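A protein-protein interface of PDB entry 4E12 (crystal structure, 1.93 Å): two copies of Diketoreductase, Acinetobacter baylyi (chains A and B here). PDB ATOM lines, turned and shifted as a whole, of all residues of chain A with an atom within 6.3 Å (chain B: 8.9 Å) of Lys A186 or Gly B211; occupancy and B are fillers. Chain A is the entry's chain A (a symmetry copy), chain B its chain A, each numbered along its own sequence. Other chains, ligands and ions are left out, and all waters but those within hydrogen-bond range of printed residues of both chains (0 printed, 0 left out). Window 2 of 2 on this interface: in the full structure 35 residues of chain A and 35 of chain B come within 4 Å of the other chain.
O of Ile B212 lies within hydrogen-bond range of N of Lys A185.
The backbone NH (N) of Ile B212 is in hydrogen-bond range of the backbone carbonyl oxygen (O) of Leu B207, 2.9 Å away. The side-chain carboxylate (OD1) of Asp B210 lies within salt-bridge range of the side-chain amino group (NZ) of Lys B254 (2.9 Å). The side-chain sulfur of Met A157 lies within hydrogen-bond range of the backbone NH of Lys A188.
Leu A184 touches Ile B212 (CA to O, 3.3 Å). Lys A185 touches Gly B211 (CB to O, 3.4 Å). Lys A185 touches Asp B214. CD of Lys A186 touches O of Asp B210, at 3.5 Å. Gly B211 touches Lys A186. Lys A186 touches Ile B212. CD1 of Ile B212 touches O of Glu A187, 3.6 Å away. Lys A188 touches Glu B206. CG of Lys A188 touches CD2 of Leu B207, at 3.9 Å. CG2 of Ile B212 touches CB of Lys A188, 3.8 Å away.
Of chain B, only Asp B210 (3.5 Å), Gly B211 (3.7 Å) and Ile B212 (3.9 Å) come within 4 Å of Lys A186. Of the printed residues of chain A, Glu B206 touches Lys A188. Of the printed residues of chain A, Asp B210 touches Lys A186 (3.5 Å). Gly B211 touches just these residues of chain A: Lys A185 and Lys A186. Printed residues of chain A within 4 Å of Ile B212: Leu A184 (3.3 Å), Lys A185 (2.6 Å), Lys A186 (3.9 Å), Glu A187 (3.6 Å) and Lys A188 (3.8 Å). Ala B213 touches none of the printed residues of chain A. Of the printed residues of chain A, Asp B214 touches Lys A185 (3.7 Å). The nearest residue of chain A that does not touch Gly B211 is Leu A184 (5.8 Å). The nearest printed residue of chain A that does not touch Glu B206 is Glu A187 (7.0 Å).
Of the 7 printed residues of chain A, 5 touch a printed residue of chain B. Hydrophobic or aromatic side chains of chain A that line the printed part of chain B: Leu A184. Of the 15 printed residues of chain B, 6 touch a printed residue of chain A. Among the printed residues, no Asp or Glu carboxylate lies within 4 Å of a Lys or Arg side-chain nitrogen of the other chain.
No position is printed for both chains. Of the 11 pairs that touch across the chains among the printed residues, none has its exchanged pair printed and touching as well.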
ATOM      1  N   MET A 157       5.727   8.647  21.400  1.00  0.00           N
ATOM      2  CA  MET A 157       4.531   8.897  22.182  1.00  0.00           C
ATOM      3  C   MET A 157       4.905   9.494  23.534  1.00  0.00           C
ATOM      4  O   MET A 157       5.520   8.820  24.364  1.00  0.00           O
ATOM      5  CB  MET A 157       3.795   7.567  22.377  1.00  0.00           C
ATOM      6  CG  MET A 157       2.420   7.648  23.001  1.00  0.00           C
ATOM      7  SD  MET A 157       1.680   6.009  23.161  1.00  0.00           S
ATOM      8  CE  MET A 157       2.528   5.430  24.625  1.00  0.00           C
ATOM      9  N   GLY A 158       4.531  10.751  23.753  1.00  0.00           N
ATOM     10  CA  GLY A 158       4.813  11.389  25.028  1.00  0.00           C
ATOM     11  C   GLY A 158       3.615  11.486  25.949  1.00  0.00           C
ATOM     12  O   GLY A 158       2.566  10.886  25.690  1.00  0.00           O
ATOM     13  N   LEU A 184       2.593   9.704  17.358  1.00  0.00           N
ATOM     14  CA  LEU A 184       1.340   9.712  18.088  1.00  0.00           C
ATOM     15  C   LEU A 184       1.171  11.037  18.802  1.00  0.00           C
ATOM     16  O   LEU A 184       2.159  11.647  19.222  1.00  0.00           O
ATOM     17  CB  LEU A 184       1.228   8.560  19.080  1.00  0.00           C
ATOM     18  CG  LEU A 184       1.123   7.136  18.538  1.00  0.00           C
ATOM     19  CD1 LEU A 184       2.448   6.653  17.966  1.00  0.00           C
ATOM     20  CD2 LEU A 184       0.700   6.249  19.694  1.00  0.00           C
ATOM     21  N   LYS A 185      -0.083  11.471  18.926  1.00  0.00           N
ATOM     22  CA  LYS A 185      -0.409  12.805  19.417  1.00  0.00           C
ATOM     23  C   LYS A 185      -0.886  12.765  20.869  1.00  0.00           C
ATOM     24  O   LYS A 185      -0.886  13.784  21.565  1.00  0.00           O
ATOM     25  CB  LYS A 185      -1.456  13.460  18.497  1.00  0.00           C
ATOM     26  CG  LYS A 185      -0.932  13.674  17.076  1.00  0.00           C
ATOM     27  CD  LYS A 185      -2.012  14.088  16.086  1.00  0.00           C
ATOM     28  CE  LYS A 185      -1.410  14.255  14.688  1.00  0.00           C
ATOM     29  NZ  LYS A 185      -2.423  14.614  13.654  1.00  0.00           N
ATOM     30  N   LYS A 186      -1.277  11.579  21.320  1.00  0.00           N
ATOM     31  CA  LYS A 186      -1.731  11.360  22.683  1.00  0.00           C
ATOM     32  C   LYS A 186      -1.336   9.945  23.078  1.00  0.00           C
ATOM     33  O   LYS A 186      -1.113   9.096  22.213  1.00  0.00           O
ATOM     34  CB  LYS A 186      -3.259  11.438  22.766  1.00  0.00           C
ATOM     35  CG  LYS A 186      -3.887  12.760  22.399  1.00  0.00           C
ATOM     36  CD  LYS A 186      -5.390  12.703  22.660  1.00  0.00           C
ATOM     37  CE  LYS A 186      -6.077  14.017  22.317  1.00  0.00           C
ATOM     38  NZ  LYS A 186      -7.545  13.969  22.575  1.00  0.00           N
ATOM     39  N   GLU A 187      -1.268   9.672  24.373  1.00  0.00           N
ATOM     40  CA  GLU A 187      -0.998   8.305  24.798  1.00  0.00           C
ATOM     41  C   GLU A 187      -2.064   7.327  24.346  1.00  0.00           C
ATOM     42  O   GLU A 187      -3.254   7.651  24.272  1.00  0.00           O
ATOM     43  CB  GLU A 187      -0.860   8.187  26.301  1.00  0.00           C
ATOM     44  CG  GLU A 187       0.406   8.728  26.867  1.00  0.00           C
ATOM     45  CD  GLU A 187       0.541   8.313  28.303  1.00  0.00           C
ATOM     46  OE1 GLU A 187      -0.458   8.441  29.045  1.00  0.00           O
ATOM     47  OE2 GLU A 187       1.621   7.824  28.680  1.00  0.00           O
ATOM     48  N   LYS A 188      -1.610   6.118  24.074  1.00  0.00           N
ATOM     49  CA  LYS A 188      -2.468   5.014  23.702  1.00  0.00           C
ATOM     50  C   LYS A 188      -1.717   3.727  24.005  1.00  0.00           C
ATOM     51  O   LYS A 188      -0.619   3.502  23.490  1.00  0.00           O
ATOM     52  CB  LYS A 188      -2.803   5.096  22.205  1.00  0.00           C
ATOM     53  CG  LYS A 188      -3.628   3.929  21.666  1.00  0.00           C
ATOM     54  CD  LYS A 188      -5.053   3.904  22.213  1.00  0.00           C
ATOM     55  CE  LYS A 188      -5.796   2.667  21.750  1.00  0.00           C
ATOM     56  NZ  LYS A 188      -5.215   1.440  22.357  1.00  0.00           N
ATOM     57  N   ALA B 204      -8.619   1.249  13.711  1.00  0.00           N
ATOM     58  CA  ALA B 204      -8.051   2.439  13.067  1.00  0.00           C
ATOM     59  C   ALA B 204      -8.927   3.676  13.348  1.00  0.00           C
ATOM     60  O   ALA B 204      -8.430   4.778  13.623  1.00  0.00           O
ATOM     61  CB  ALA B 204      -7.937   2.204  11.559  1.00  0.00           C
ATOM     62  N   ALA B 205     -10.233   3.489  13.242  1.00  0.00           N
ATOM     63  CA  ALA B 205     -11.161   4.593  13.419  1.00  0.00           C
ATOM     64  C   ALA B 205     -11.070   5.164  14.837  1.00  0.00           C
ATOM     65  O   ALA B 205     -11.081   6.386  15.017  1.00  0.00           O
ATOM     66  CB  ALA B 205     -12.578   4.158  13.093  1.00  0.00           C
ATOM     67  N   GLU B 206     -10.975   4.289  15.831  1.00  0.00           N
ATOM     68  CA  GLU B 206     -10.777   4.723  17.218  1.00  0.00           C
ATOM     69  C   GLU B 206      -9.502   5.550  17.377  1.00  0.00           C
ATOM     70  O   GLU B 206      -9.514   6.602  18.023  1.00  0.00           O
ATOM     71  CB  GLU B 206     -10.730   3.517  18.161  1.00  0.00           C
ATOM     72  CG  GLU B 206     -10.466   3.869  19.626  1.00  0.00           C
ATOM     73  CD  GLU B 206      -9.004   4.218  19.926  1.00  0.00           C
ATOM     74  OE1 GLU B 206      -8.753   5.019  20.848  1.00  0.00           O
ATOM     75  OE2 GLU B 206      -8.098   3.680  19.257  1.00  0.00           O
ATOM     76  N   LEU B 207      -8.397   5.088  16.807  1.00  0.00           N
ATOM     77  CA  LEU B 207      -7.160   5.876  16.845  1.00  0.00           C
ATOM     78  C   LEU B 207      -7.370   7.244  16.208  1.00  0.00           C
ATOM     79  O   LEU B 207      -6.817   8.244  16.670  1.00  0.00           O
ATOM     80  CB  LEU B 207      -6.036   5.184  16.074  1.00  0.00           C
ATOM     81  CG  LEU B 207      -5.550   3.819  16.550  1.00  0.00           C
ATOM     82  CD1 LEU B 207      -4.510   3.296  15.546  1.00  0.00           C
ATOM     83  CD2 LEU B 207      -4.946   3.990  17.943  1.00  0.00           C
ATOM     84  N   LEU B 208      -8.132   7.305  15.116  1.00  0.00           N
ATOM     85  CA  LEU B 208      -8.331   8.598  14.467  1.00  0.00           C
ATOM     86  C   LEU B 208      -9.226   9.464  15.332  1.00  0.00           C
ATOM     87  O   LEU B 208      -8.896  10.613  15.638  1.00  0.00           O
ATOM     88  CB  LEU B 208      -8.974   8.447  13.087  1.00  0.00           C
ATOM     89  CG  LEU B 208      -9.271   9.752  12.325  1.00  0.00           C
ATOM     90  CD1 LEU B 208      -8.008  10.597  12.117  1.00  0.00           C
ATOM     91  CD2 LEU B 208      -9.939   9.420  10.998  1.00  0.00           C
ATOM     92  N   VAL B 209     -10.372   8.907  15.699  1.00  0.00           N
ATOM     93  CA  VAL B 209     -11.392   9.650  16.432  1.00  0.00           C
ATOM     94  C   VAL B 209     -10.932  10.102  17.813  1.00  0.00           C
ATOM     95  O   VAL B 209     -11.392  11.132  18.325  1.00  0.00           O
ATOM     96  CB  VAL B 209     -12.683   8.851  16.554  1.00  0.00           C
ATOM     97  CG1 VAL B 209     -13.666   9.587  17.435  1.00  0.00           C
ATOM     98  CG2 VAL B 209     -13.299   8.679  15.188  1.00  0.00           C
ATOM     99  N   ASP B 210     -10.028   9.353  18.429  1.00  0.00           N
ATOM    100  CA  ASP B 210      -9.542   9.746  19.753  1.00  0.00           C
ATOM    101  C   ASP B 210      -8.322  10.647  19.669  1.00  0.00           C
ATOM    102  O   ASP B 210      -7.705  10.957  20.692  1.00  0.00           O
ATOM    103  CB  ASP B 210      -9.252   8.540  20.643  1.00  0.00           C
ATOM    104  CG  ASP B 210     -10.520   7.806  21.089  1.00  0.00           C
ATOM    105  OD1 ASP B 210     -11.623   8.399  21.094  1.00  0.00           O
ATOM    106  OD2 ASP B 210     -10.417   6.624  21.446  1.00  0.00           O
ATOM    107  N   GLY B 211      -7.972  11.058  18.455  1.00  0.00           N
ATOM    108  CA  GLY B 211      -6.863  11.968  18.263  1.00  0.00           C
ATOM    109  C   GLY B 211      -5.473  11.397  18.501  1.00  0.00           C
ATOM    110  O   GLY B 211      -4.551  12.147  18.822  1.00  0.00           O
ATOM    111  N   ILE B 212      -5.305  10.084  18.344  1.00  0.00           N
ATOM    112  CA  ILE B 212      -4.009   9.464  18.598  1.00  0.00           C
ATOM    113  C   ILE B 212      -3.046   9.717  17.443  1.00  0.00           C
ATOM    114  O   ILE B 212      -1.879  10.039  17.671  1.00  0.00           O
ATOM    115  CB  ILE B 212      -4.136   7.932  18.784  1.00  0.00           C
ATOM    116  CG1 ILE B 212      -5.201   7.584  19.820  1.00  0.00           C
ATOM    117  CG2 ILE B 212      -2.795   7.317  19.163  1.00  0.00           C
ATOM    118  CD1 ILE B 212      -4.966   8.186  21.199  1.00  0.00           C
ATOM    119  N   ALA B 213      -3.526   9.567  16.205  1.00  0.00           N
ATOM    120  CA  ALA B 213      -2.671   9.666  15.027  1.00  0.00           C
ATOM    121  C   ALA B 213      -3.504  10.081  13.821  1.00  0.00           C
ATOM    122  O   ALA B 213      -4.728   9.912  13.828  1.00  0.00           O
ATOM    123  CB  ALA B 213      -2.010   8.315  14.754  1.00  0.00           C
ATOM    124  N   ASP B 214      -2.867  10.622  12.785  1.00  0.00           N
ATOM    125  CA  ASP B 214      -3.637  11.008  11.593  1.00  0.00           C
ATOM    126  C   ASP B 214      -3.782   9.789  10.673  1.00  0.00           C
ATOM    127  O   ASP B 214      -3.110   8.775  10.892  1.00  0.00           O
ATOM    128  CB  ASP B 214      -3.010  12.219  10.889  1.00  0.00           C
ATOM    129  CG  ASP B 214      -1.613  11.953  10.390  1.00  0.00           C
ATOM    130  OD1 ASP B 214      -0.847  12.923  10.202  1.00  0.00           O
ATOM    131  OD2 ASP B 214      -1.284  10.775  10.168  1.00  0.00           O
ATOM    132  N   ILE B 218      -1.480   6.216  10.491  1.00  0.00           N
ATOM    133  CA  ILE B 218      -2.078   4.923  10.827  1.00  0.00           C
ATOM    134  C   ILE B 218      -1.861   3.964   9.653  1.00  0.00           C
ATOM    135  O   ILE B 218      -1.441   2.814   9.839  1.00  0.00           O
ATOM    136  CB  ILE B 218      -3.572   5.119  11.175  1.00  0.00           C
ATOM    137  CG1 ILE B 218      -3.677   6.064  12.385  1.00  0.00           C
ATOM    138  CG2 ILE B 218      -4.256   3.793  11.415  1.00  0.00           C
ATOM    139  CD1 ILE B 218      -5.078   6.479  12.754  1.00  0.00           C
ATOM    140  N   LYS B 254     -18.019   3.912  20.216  1.00  0.00           N
ATOM    141  CA  LYS B 254     -16.829   4.441  19.571  1.00  0.00           C
ATOM    142  C   LYS B 254     -17.082   4.501  18.071  1.00  0.00           C
ATOM    143  O   LYS B 254     -16.696   5.458  17.402  1.00  0.00           O
ATOM    144  CB  LYS B 254     -15.607   3.571  19.856  1.00  0.00           C
ATOM    145  CG  LYS B 254     -14.328   4.122  19.280  1.00  0.00           C
ATOM    146  CD  LYS B 254     -14.018   5.504  19.885  1.00  0.00           C
ATOM    147  CE  LYS B 254     -13.928   5.410  21.399  1.00  0.00           C
ATOM    148  NZ  LYS B 254     -13.777   6.747  22.047  1.00  0.00           N
ATOM    149  N   GLU B 257     -19.232   7.358  17.069  1.00  0.00           N
ATOM    150  CA  GLU B 257     -18.441   8.567  17.137  1.00  0.00           C
ATOM    151  C   GLU B 257     -17.680   8.756  15.815  1.00  0.00           C
ATOM    152  O   GLU B 257     -17.578   9.871  15.305  1.00  0.00           O
ATOM    153  CB  GLU B 257     -17.498   8.466  18.330  1.00  0.00           C
ATOM    154  CG  GLU B 257     -16.662   9.691  18.608  1.00  0.00           C
ATOM    155  CD  GLU B 257     -15.944   9.606  19.963  1.00  0.00           C
ATOM    156  OE1 GLU B 257     -16.321   8.747  20.799  1.00  0.00           O
ATOM    157  OE2 GLU B 257     -15.003  10.401  20.193  1.00  0.00           O
ATOM    158  N   TYR B 261     -17.895  11.560  12.767  1.00  0.00           N
ATOM    159  CA  TYR B 261     -16.654  12.156  12.278  1.00  0.00           C
ATOM    160  C   TYR B 261     -16.628  12.135  10.756  1.00  0.00           C
ATOM    161  O   TYR B 261     -16.265  13.118  10.099  1.00  0.00           O
ATOM    162  CB  TYR B 261     -15.439  11.389  12.829  1.00  0.00           C
ATOM    163  CG  TYR B 261     -14.103  11.940  12.402  1.00  0.00           C
ATOM    164  CD1 TYR B 261     -13.420  12.869  13.194  1.00  0.00           C
ATOM    165  CD2 TYR B 261     -13.509  11.536  11.209  1.00  0.00           C
ATOM    166  CE1 TYR B 261     -12.183  13.374  12.797  1.00  0.00           C
ATOM    167  CE2 TYR B 261     -12.272  12.034  10.808  1.00  0.00           C
ATOM    168  CZ  TYR B 261     -11.615  12.950  11.600  1.00  0.00           C
ATOM    169  OH  TYR B 261     -10.393  13.446  11.194  1.00  0.00           O
